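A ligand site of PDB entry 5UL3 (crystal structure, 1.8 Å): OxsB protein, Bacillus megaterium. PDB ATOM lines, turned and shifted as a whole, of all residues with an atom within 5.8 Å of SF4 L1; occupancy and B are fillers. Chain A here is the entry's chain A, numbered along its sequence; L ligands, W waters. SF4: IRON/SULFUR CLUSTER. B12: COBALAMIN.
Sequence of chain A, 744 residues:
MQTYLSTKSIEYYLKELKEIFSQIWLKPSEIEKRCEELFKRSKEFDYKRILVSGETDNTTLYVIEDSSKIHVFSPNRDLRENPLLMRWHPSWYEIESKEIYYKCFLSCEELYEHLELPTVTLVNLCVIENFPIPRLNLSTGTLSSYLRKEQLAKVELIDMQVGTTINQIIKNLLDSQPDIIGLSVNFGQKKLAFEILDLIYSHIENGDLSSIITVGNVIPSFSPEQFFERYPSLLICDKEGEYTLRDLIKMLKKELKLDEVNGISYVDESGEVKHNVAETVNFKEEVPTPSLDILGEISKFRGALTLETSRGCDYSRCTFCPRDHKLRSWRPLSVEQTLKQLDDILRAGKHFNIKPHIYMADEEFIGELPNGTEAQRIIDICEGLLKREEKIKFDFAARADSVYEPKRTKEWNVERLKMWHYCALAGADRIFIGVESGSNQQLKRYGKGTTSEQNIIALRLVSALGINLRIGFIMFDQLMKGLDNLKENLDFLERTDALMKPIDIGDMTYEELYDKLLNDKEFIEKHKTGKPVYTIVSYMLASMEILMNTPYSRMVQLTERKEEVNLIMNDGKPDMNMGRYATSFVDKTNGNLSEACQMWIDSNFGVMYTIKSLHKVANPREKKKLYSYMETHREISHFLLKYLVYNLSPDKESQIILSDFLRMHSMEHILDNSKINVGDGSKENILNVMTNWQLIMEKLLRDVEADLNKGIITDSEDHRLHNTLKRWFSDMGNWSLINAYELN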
ATOM      1  N   CYS A 313     -29.437  11.523  25.469  1.00  0.00           N
ATOM      2  CA  CYS A 313     -28.966  12.551  24.554  1.00  0.00           C
ATOM      3  C   CYS A 313     -29.945  12.593  23.395  1.00  0.00           C
ATOM      4  O   CYS A 313     -30.165  11.567  22.752  1.00  0.00           O
ATOM      5  CB  CYS A 313     -27.571  12.223  24.043  1.00  0.00           C
ATOM      6  SG  CYS A 313     -26.939  13.480  22.863  1.00  0.00           S
ATOM      7  N   TYR A 315     -29.503  14.138  20.650  1.00  0.00           N
ATOM      8  CA  TYR A 315     -28.752  14.089  19.394  1.00  0.00           C
ATOM      9  C   TYR A 315     -28.367  12.662  19.041  1.00  0.00           C
ATOM     10  O   TYR A 315     -28.816  12.115  18.029  1.00  0.00           O
ATOM     11  CB  TYR A 315     -27.511  14.977  19.492  1.00  0.00           C
ATOM     12  CG  TYR A 315     -26.725  15.054  18.200  1.00  0.00           C
ATOM     13  CD1 TYR A 315     -27.289  15.616  17.055  1.00  0.00           C
ATOM     14  CD2 TYR A 315     -25.413  14.597  18.150  1.00  0.00           C
ATOM     15  CE1 TYR A 315     -26.548  15.710  15.867  1.00  0.00           C
ATOM     16  CE2 TYR A 315     -24.675  14.681  16.935  1.00  0.00           C
ATOM     17  CZ  TYR A 315     -25.258  15.225  15.827  1.00  0.00           C
ATOM     18  OH  TYR A 315     -24.502  15.298  14.653  1.00  0.00           O
ATOM     19  N   SER A 316     -27.494  12.046  19.861  1.00  0.00           N
ATOM     20  CA  SER A 316     -27.216  10.618  19.834  1.00  0.00           C
ATOM     21  C   SER A 316     -26.584  10.155  18.521  1.00  0.00           C
ATOM     22  O   SER A 316     -26.596   8.962  18.215  1.00  0.00           O
ATOM     23  CB  SER A 316     -28.473   9.794  20.127  1.00  0.00           C
ATOM     24  OG  SER A 316     -28.742   9.699  21.526  1.00  0.00           O
ATOM     25  N   ARG A 317     -25.974  11.056  17.743  1.00  0.00           N
ATOM     26  CA  ARG A 317     -25.452  10.722  16.433  1.00  0.00           C
ATOM     27  C   ARG A 317     -23.944  10.719  16.329  1.00  0.00           C
ATOM     28  O   ARG A 317     -23.419  10.392  15.239  1.00  0.00           O
ATOM     29  CB  ARG A 317     -26.014  11.688  15.392  1.00  0.00           C
ATOM     30  CG  ARG A 317     -27.462  11.464  15.117  1.00  0.00           C
ATOM     31  CD  ARG A 317     -27.932  12.536  14.178  1.00  0.00           C
ATOM     32  NE  ARG A 317     -29.271  12.326  13.641  1.00  0.00           N
ATOM     33  CZ  ARG A 317     -30.400  12.577  14.295  1.00  0.00           C
ATOM     34  NH1 ARG A 317     -30.396  13.007  15.566  1.00  0.00           N
ATOM     35  NH2 ARG A 317     -31.552  12.389  13.687  1.00  0.00           N
ATOM     36  N   CYS A 318     -23.227  11.086  17.380  1.00  0.00           N
ATOM     37  CA  CYS A 318     -21.765  11.068  17.318  1.00  0.00           C
ATOM     38  C   CYS A 318     -21.292   9.629  17.126  1.00  0.00           C
ATOM     39  O   CYS A 318     -21.748   8.723  17.823  1.00  0.00           O
ATOM     40  CB  CYS A 318     -21.162  11.691  18.575  1.00  0.00           C
ATOM     41  SG  CYS A 318     -21.795  13.365  18.821  1.00  0.00           S
ATOM     42  N   PHE A 320     -18.618   7.915  17.629  1.00  0.00           N
ATOM     43  CA  PHE A 320     -17.796   7.279  18.640  1.00  0.00           C
ATOM     44  C   PHE A 320     -18.548   7.069  19.960  1.00  0.00           C
ATOM     45  O   PHE A 320     -17.968   6.520  20.911  1.00  0.00           O
ATOM     46  CB  PHE A 320     -16.548   8.131  18.902  1.00  0.00           C
ATOM     47  CG  PHE A 320     -16.877   9.545  19.313  1.00  0.00           C
ATOM     48  CD1 PHE A 320     -17.163   9.850  20.647  1.00  0.00           C
ATOM     49  CD2 PHE A 320     -16.983  10.557  18.363  1.00  0.00           C
ATOM     50  CE1 PHE A 320     -17.500  11.133  21.026  1.00  0.00           C
ATOM     51  CE2 PHE A 320     -17.321  11.840  18.728  1.00  0.00           C
ATOM     52  CZ  PHE A 320     -17.585  12.144  20.067  1.00  0.00           C
ATOM     53  N   CYS A 321     -19.794   7.493  20.053  1.00  0.00           N
ATOM     54  CA  CYS A 321     -20.534   7.481  21.324  1.00  0.00           C
ATOM     55  C   CYS A 321     -21.642   6.433  21.257  1.00  0.00           C
ATOM     56  O   CYS A 321     -22.688   6.678  20.642  1.00  0.00           O
ATOM     57  CB  CYS A 321     -21.110   8.880  21.578  1.00  0.00           C
ATOM     58  SG  CYS A 321     -21.941   9.117  23.202  1.00  0.00           S
ATOM     59  N   ARG A 323     -24.950   4.441  21.961  1.00  0.00           N
ATOM     60  CA  ARG A 323     -26.186   4.890  22.587  1.00  0.00           C
ATOM     61  C   ARG A 323     -27.018   3.772  23.209  1.00  0.00           C
ATOM     62  O   ARG A 323     -28.075   4.045  23.776  1.00  0.00           O
ATOM     63  CB  ARG A 323     -27.023   5.688  21.573  1.00  0.00           C
ATOM     64  CG  ARG A 323     -26.257   6.882  20.942  1.00  0.00           C
ATOM     65  CD  ARG A 323     -25.586   7.776  22.022  1.00  0.00           C
ATOM     66  NE  ARG A 323     -26.536   8.225  23.042  1.00  0.00           N
ATOM     67  CZ  ARG A 323     -26.177   8.616  24.268  1.00  0.00           C
ATOM     68  NH1 ARG A 323     -27.105   9.008  25.145  1.00  0.00           N
ATOM     69  NH2 ARG A 323     -24.892   8.594  24.616  1.00  0.00           N
ATOM     70  N   GLU A 363     -25.349  13.712  30.502  1.00  0.00           N
ATOM     71  CA  GLU A 363     -24.728  13.741  29.173  1.00  0.00           C
ATOM     72  C   GLU A 363     -25.056  15.040  28.455  1.00  0.00           C
ATOM     73  O   GLU A 363     -24.220  15.582  27.723  1.00  0.00           O
ATOM     74  CB  GLU A 363     -25.224  12.551  28.351  1.00  0.00           C
ATOM     75  CG  GLU A 363     -24.633  11.212  28.771  1.00  0.00           C
ATOM     76  CD  GLU A 363     -25.043  10.101  27.830  1.00  0.00           C
ATOM     77  OE1 GLU A 363     -26.276   9.923  27.658  1.00  0.00           O
ATOM     78  OE2 GLU A 363     -24.141   9.468  27.225  1.00  0.00           O
ATOM     79  N   GLU A 364     -26.269  15.544  28.657  1.00  0.00           N
ATOM     80  CA  GLU A 364     -26.811  16.689  27.923  1.00  0.00           C
ATOM     81  C   GLU A 364     -27.634  17.508  28.907  1.00  0.00           C
ATOM     82  O   GLU A 364     -28.834  17.268  29.089  1.00  0.00           O
ATOM     83  CB  GLU A 364     -27.658  16.238  26.725  1.00  0.00           C
ATOM     84  CG  GLU A 364     -28.302  17.389  25.960  1.00  0.00           C
ATOM     85  CD  GLU A 364     -29.128  16.926  24.767  1.00  0.00           C
ATOM     86  OE1 GLU A 364     -29.538  15.743  24.718  1.00  0.00           O
ATOM     87  OE2 GLU A 364     -29.362  17.770  23.870  1.00  0.00           O
ATOM     88  N   ARG A 399     -22.865  20.176  24.019  1.00  0.00           N
ATOM     89  CA  ARG A 399     -22.375  20.225  22.647  1.00  0.00           C
ATOM     90  C   ARG A 399     -22.139  21.658  22.212  1.00  0.00           C
ATOM     91  O   ARG A 399     -22.818  22.590  22.672  1.00  0.00           O
ATOM     92  CB  ARG A 399     -23.378  19.592  21.662  1.00  0.00           C
ATOM     93  CG  ARG A 399     -24.108  18.370  22.119  1.00  0.00           C
ATOM     94  CD  ARG A 399     -24.889  17.733  20.940  1.00  0.00           C
ATOM     95  NE  ARG A 399     -25.825  18.620  20.262  1.00  0.00           N
ATOM     96  CZ  ARG A 399     -27.106  18.752  20.587  1.00  0.00           C
ATOM     97  NH1 ARG A 399     -27.888  19.587  19.908  1.00  0.00           N
ATOM     98  NH2 ARG A 399     -27.616  18.062  21.606  1.00  0.00           N
ATOM     99  N   LYS A 448     -20.392  14.689  14.323  1.00  0.00           N
ATOM    100  CA  LYS A 448     -20.648  15.782  15.260  1.00  0.00           C
ATOM    101  C   LYS A 448     -21.643  16.788  14.729  1.00  0.00           C
ATOM    102  O   LYS A 448     -22.289  17.487  15.532  1.00  0.00           O
ATOM    103  CB  LYS A 448     -19.337  16.501  15.610  1.00  0.00           C
ATOM    104  CG  LYS A 448     -18.313  15.681  16.390  1.00  0.00           C
ATOM    105  CD  LYS A 448     -18.845  15.214  17.755  1.00  0.00           C
ATOM    106  CE  LYS A 448     -19.319  16.372  18.614  1.00  0.00           C
ATOM    107  NZ  LYS A 448     -19.560  15.914  20.017  1.00  0.00           N
HETATM  108 FE1  SF4 L   1     -22.533  13.058  20.917  1.00  0.00          FE
HETATM  109 FE2  SF4 L   1     -22.286  13.970  23.467  1.00  0.00          FE
HETATM  110 FE3  SF4 L   1     -22.608  11.249  22.915  1.00  0.00          FE
HETATM  111 FE4  SF4 L   1     -24.714  12.963  22.585  1.00  0.00          FE
HETATM  112  S1  SF4 L   1     -23.655  12.448  24.571  1.00  0.00           S
HETATM  113  S2  SF4 L   1     -24.047  11.328  21.117  1.00  0.00           S
HETATM  114  S3  SF4 L   1     -23.604  14.827  21.794  1.00  0.00           S
HETATM  115  S4  SF4 L   1     -20.823  12.604  22.352  1.00  0.00           S
HETATM  116 CO   B12 L   2     -17.533   8.593  32.188  1.00  0.00          CO
HETATM  117  N21 B12 L   2     -18.625   7.935  30.801  1.00  0.00           N
HETATM  118  N22 B12 L   2     -16.031   7.686  31.408  1.00  0.00           N
HETATM  119  N23 B12 L   2     -16.651   9.085  33.808  1.00  0.00           N
HETATM  120  N24 B12 L   2     -19.134   9.353  32.826  1.00  0.00           N
HETATM  121  C1  B12 L   2     -20.079   8.125  30.930  1.00  0.00           C
HETATM  122  C20 B12 L   2     -20.638   6.960  31.737  1.00  0.00           C
HETATM  123  C2  B12 L   2     -20.583   8.169  29.420  1.00  0.00           C
HETATM  124  C25 B12 L   2     -22.025   7.665  29.214  1.00  0.00           C
HETATM  125  C26 B12 L   2     -20.378   9.590  28.846  1.00  0.00           C
HETATM  126  C27 B12 L   2     -20.291   9.675  27.290  1.00  0.00           C
HETATM  127  O28 B12 L   2     -19.200   9.669  26.699  1.00  0.00           O
HETATM  128  N29 B12 L   2     -21.453   9.748  26.663  1.00  0.00           N
HETATM  129  C3  B12 L   2     -19.530   7.220  28.747  1.00  0.00           C
HETATM  130  C30 B12 L   2     -19.935   5.736  28.719  1.00  0.00           C
HETATM  131  C31 B12 L   2     -20.053   5.159  27.293  1.00  0.00           C
HETATM  132  C32 B12 L   2     -21.420   5.390  26.693  1.00  0.00           C
HETATM  133  O34 B12 L   2     -21.573   6.176  25.739  1.00  0.00           O
HETATM  134  N33 B12 L   2     -22.422   4.725  27.239  1.00  0.00           N
HETATM  135  C4  B12 L   2     -18.328   7.433  29.648  1.00  0.00           C
HETATM  136  C5  B12 L   2     -16.947   7.089  29.232  1.00  0.00           C
HETATM  137  C35 B12 L   2     -16.833   6.644  27.799  1.00  0.00           C
HETATM  138  C6  B12 L   2     -15.891   7.203  30.115  1.00  0.00           C
HETATM  139  C7  B12 L   2     -14.420   6.906  29.830  1.00  0.00           C
HETATM  140  C36 B12 L   2     -14.155   5.530  29.184  1.00  0.00           C
HETATM  141  C37 B12 L   2     -13.864   8.080  28.995  1.00  0.00           C
HETATM  142  C38 B12 L   2     -12.465   7.732  28.477  1.00  0.00           C
HETATM  143  O39 B12 L   2     -11.496   7.738  29.237  1.00  0.00           O
HETATM  144  N40 B12 L   2     -12.367   7.433  27.185  1.00  0.00           N
HETATM  145  C8  B12 L   2     -13.784   6.940  31.246  1.00  0.00           C
HETATM  146  C41 B12 L   2     -13.660   5.566  31.925  1.00  0.00           C
HETATM  147  C42 B12 L   2     -12.758   5.593  33.169  1.00  0.00           C
HETATM  148  C43 B12 L   2     -12.611   4.268  33.886  1.00  0.00           C
HETATM  149  O44 B12 L   2     -13.527   3.822  34.596  1.00  0.00           O
HETATM  150  N45 B12 L   2     -11.461   3.639  33.723  1.00  0.00           N
HETATM  151  C9  B12 L   2     -14.819   7.729  32.012  1.00  0.00           C
HETATM  152  C10 B12 L   2     -14.449   8.408  33.180  1.00  0.00           C
HETATM  153  C11 B12 L   2     -15.332   9.105  33.974  1.00  0.00           C
HETATM  154  C12 B12 L   2     -14.926   9.864  35.215  1.00  0.00           C
HETATM  155  C46 B12 L   2     -14.635  11.324  34.808  1.00  0.00           C
HETATM  156  C47 B12 L   2     -13.677   9.263  35.872  1.00  0.00           C
HETATM  157  C13 B12 L   2     -16.249   9.826  36.074  1.00  0.00           C
HETATM  158  C48 B12 L   2     -16.461   8.586  36.972  1.00  0.00           C
HETATM  159  C49 B12 L   2     -16.108   8.845  38.436  1.00  0.00           C
HETATM  160  C50 B12 L   2     -16.761   7.956  39.475  1.00  0.00           C
HETATM  161  O51 B12 L   2     -17.821   7.360  39.236  1.00  0.00           O
HETATM  162  N52 B12 L   2     -16.135   7.862  40.638  1.00  0.00           N
HETATM  163  C14 B12 L   2     -17.263   9.691  34.930  1.00  0.00           C
HETATM  164  C15 B12 L   2     -18.538  10.168  35.047  1.00  0.00           C
HETATM  165  C53 B12 L   2     -18.978  10.894  36.283  1.00  0.00           C
HETATM  166  C16 B12 L   2     -19.500   9.988  33.899  1.00  0.00           C
HETATM  167  C17 B12 L   2     -20.908  10.539  33.787  1.00  0.00           C
HETATM  168  C54 B12 L   2     -20.792  12.023  33.392  1.00  0.00           C
HETATM  169  C55 B12 L   2     -21.899  10.364  34.975  1.00  0.00           C
HETATM  170  C56 B12 L   2     -22.007   8.944  35.524  1.00  0.00           C
HETATM  171  C57 B12 L   2     -23.316   8.912  36.304  1.00  0.00           C
HETATM  172  O58 B12 L   2     -23.371   9.294  37.469  1.00  0.00           O
HETATM  173  N59 B12 L   2     -24.373   8.485  35.641  1.00  0.00           N
HETATM  174  C18 B12 L   2     -21.456   9.644  32.651  1.00  0.00           C
HETATM  175  C60 B12 L   2     -22.650  10.248  31.909  1.00  0.00           C
HETATM  176  C61 B12 L   2     -23.951   9.655  32.416  1.00  0.00           C
HETATM  177  O63 B12 L   2     -24.044   8.456  32.673  1.00  0.00           O
HETATM  178  N62 B12 L   2     -24.963  10.503  32.566  1.00  0.00           N
HETATM  179  C19 B12 L   2     -20.207   9.417  31.784  1.00  0.00           C
HETATM  180  C1P B12 L   2     -25.725   8.509  36.189  1.00  0.00           C
HETATM  181  C2P B12 L   2     -26.160   7.094  36.682  1.00  0.00           C
HETATM  182  C3P B12 L   2     -27.548   7.133  37.277  1.00  0.00           C
HETATM  183  O3  B12 L   2     -26.221   6.220  35.548  1.00  0.00           O
HETATM  184  O4  B12 L   2     -24.190   4.712  36.146  1.00  0.00           O
HETATM  185  O5  B12 L   2     -25.563   4.355  34.044  1.00  0.00           O
HETATM  186  P   B12 L   2     -25.531   4.789  35.504  1.00  0.00           P
HETATM  187  O2  B12 L   2     -26.584   3.874  36.303  1.00  0.00           O
HETATM  188  C3R B12 L   2     -27.836   3.437  35.819  1.00  0.00           C
HETATM  189  C2R B12 L   2     -27.760   2.179  34.934  1.00  0.00           C
HETATM  190  O7R B12 L   2     -26.459   1.909  34.433  1.00  0.00           O
HETATM  191  C1R B12 L   2     -28.238   1.093  35.887  1.00  0.00           C
HETATM  192  O6R B12 L   2     -29.188   1.707  36.726  1.00  0.00           O
HETATM  193  C4R B12 L   2     -28.761   3.056  36.990  1.00  0.00           C
HETATM  194  C5R B12 L   2     -29.966   3.941  37.176  1.00  0.00           C
HETATM  195  O8R B12 L   2     -30.823   3.913  36.019  1.00  0.00           O
HETATM  196  N1B B12 L   2     -27.194   0.463  36.717  1.00  0.00           N
HETATM  197  C8B B12 L   2     -27.439  -0.689  37.439  1.00  0.00           C
HETATM  198  C2B B12 L   2     -25.982   0.931  37.127  1.00  0.00           C
HETATM  199  N3B B12 L   2     -25.416   0.182  38.049  1.00  0.00           N
HETATM  200  C9B B12 L   2     -26.327  -0.853  38.265  1.00  0.00           C
HETATM  201  C4B B12 L   2     -26.271  -1.924  39.144  1.00  0.00           C
HETATM  202  C5B B12 L   2     -27.325  -2.832  39.196  1.00  0.00           C
HETATM  203  C5M B12 L   2     -27.241  -4.003  40.145  1.00  0.00           C
HETATM  204  C6B B12 L   2     -28.464  -2.646  38.372  1.00  0.00           C
HETATM  205  C6M B12 L   2     -29.641  -3.593  38.446  1.00  0.00           C
HETATM  206  C7B B12 L   2     -28.506  -1.566  37.492  1.00  0.00           C
HETATM  207  O   HOH W   1     -18.788  11.266  24.554  1.00  0.00           O
HETATM  208  O   HOH W   2     -18.348  15.053  22.556  1.00  0.00           O
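The side-chain hydroxyl (OG) of Ser 316 sits at hydrogen-bond distance from the guanidinium group (NE) of Arg 323 (3.1 Å). SG of Cys 318 lies close to NZ of Lys 448. The guanidinium group (NH1) of Arg 323 lies within salt-bridge range of the side-chain carboxylate (OE1) of Glu 363, at 2.8 Å. The guanidinium group (NH2) of Arg 399 is in salt-bridge range of the side-chain carboxylate (OE2) of Glu 364, 2.9 Å away. The guanidinium group of Arg 317 lies within hydrogen-bond range of the backbone carbonyl oxygen of Tyr 315 (3.1 Å). The side-chain sulfur (SG) of Cys 313 lies close to the backbone NH (N) of Tyr 315 (3.5 Å). NH2 of Arg 323 sits close to SG of Cys 321, 3.3 Å away. The backbone carbonyl oxygen (O) of Cys 313 sits at hydrogen-bond distance from the side-chain hydroxyl (OG) of Ser 316 (2.6 Å).
Water W1 lies within hydrogen-bond range of O28 of B12 L2 (2.7 Å) and S4 of SF4 L1 (3.3 Å). Water W2 lies within hydrogen-bond range of the side-chain amino group of Lys 448 (2.9 Å) and a sulfur (S4) of SF4 L1 (3.5 Å).
N of Arg 317 touches S2 of SF4 L1, 3.9 Å away. CE1 of Phe 320 touches S4 of SF4 L1 (3.9 Å). NH2 of Arg 323 touches FE3 of SF4 L1 (3.9 Å). Arg 399 touches SF4 L1 (CD to S3, 3.3 Å). Hydrophobic or aromatic side chains that line SF4 L1: Phe 320. Eight residues have an atom within 4 Å of SF4 L1: Cys 313, Ser 316, Arg 317, Cys 318, Phe 320, Cys 321, Arg 323 and Arg 399. The nearest printed residue that does not touch SF4 L1 is Glu 363 (4.02 Å).
The side-chain carboxylate of Glu 363 sits at hydrogen-bond distance from a nitrogen (N29) of B12 L2, 2.8 Å away. The backbone NH (N) of Ser 316 lies close to a sulfur (S2) of SF4 L1, 3.7 Å away. The side-chain sulfur of Cys 318 binds an iron atom (FE1) of SF4 L1 (2.2 Å). An iron atom (FE4) of SF4 L1 is bound by the side-chain sulfur (SG) of Cys 313, at 2.3 Å. FE3 of SF4 L1 is bound by SG of Cys 321 (2.3 Å). N29 of B12 L2 lies close to SG of Cys 321 (3.6 Å).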
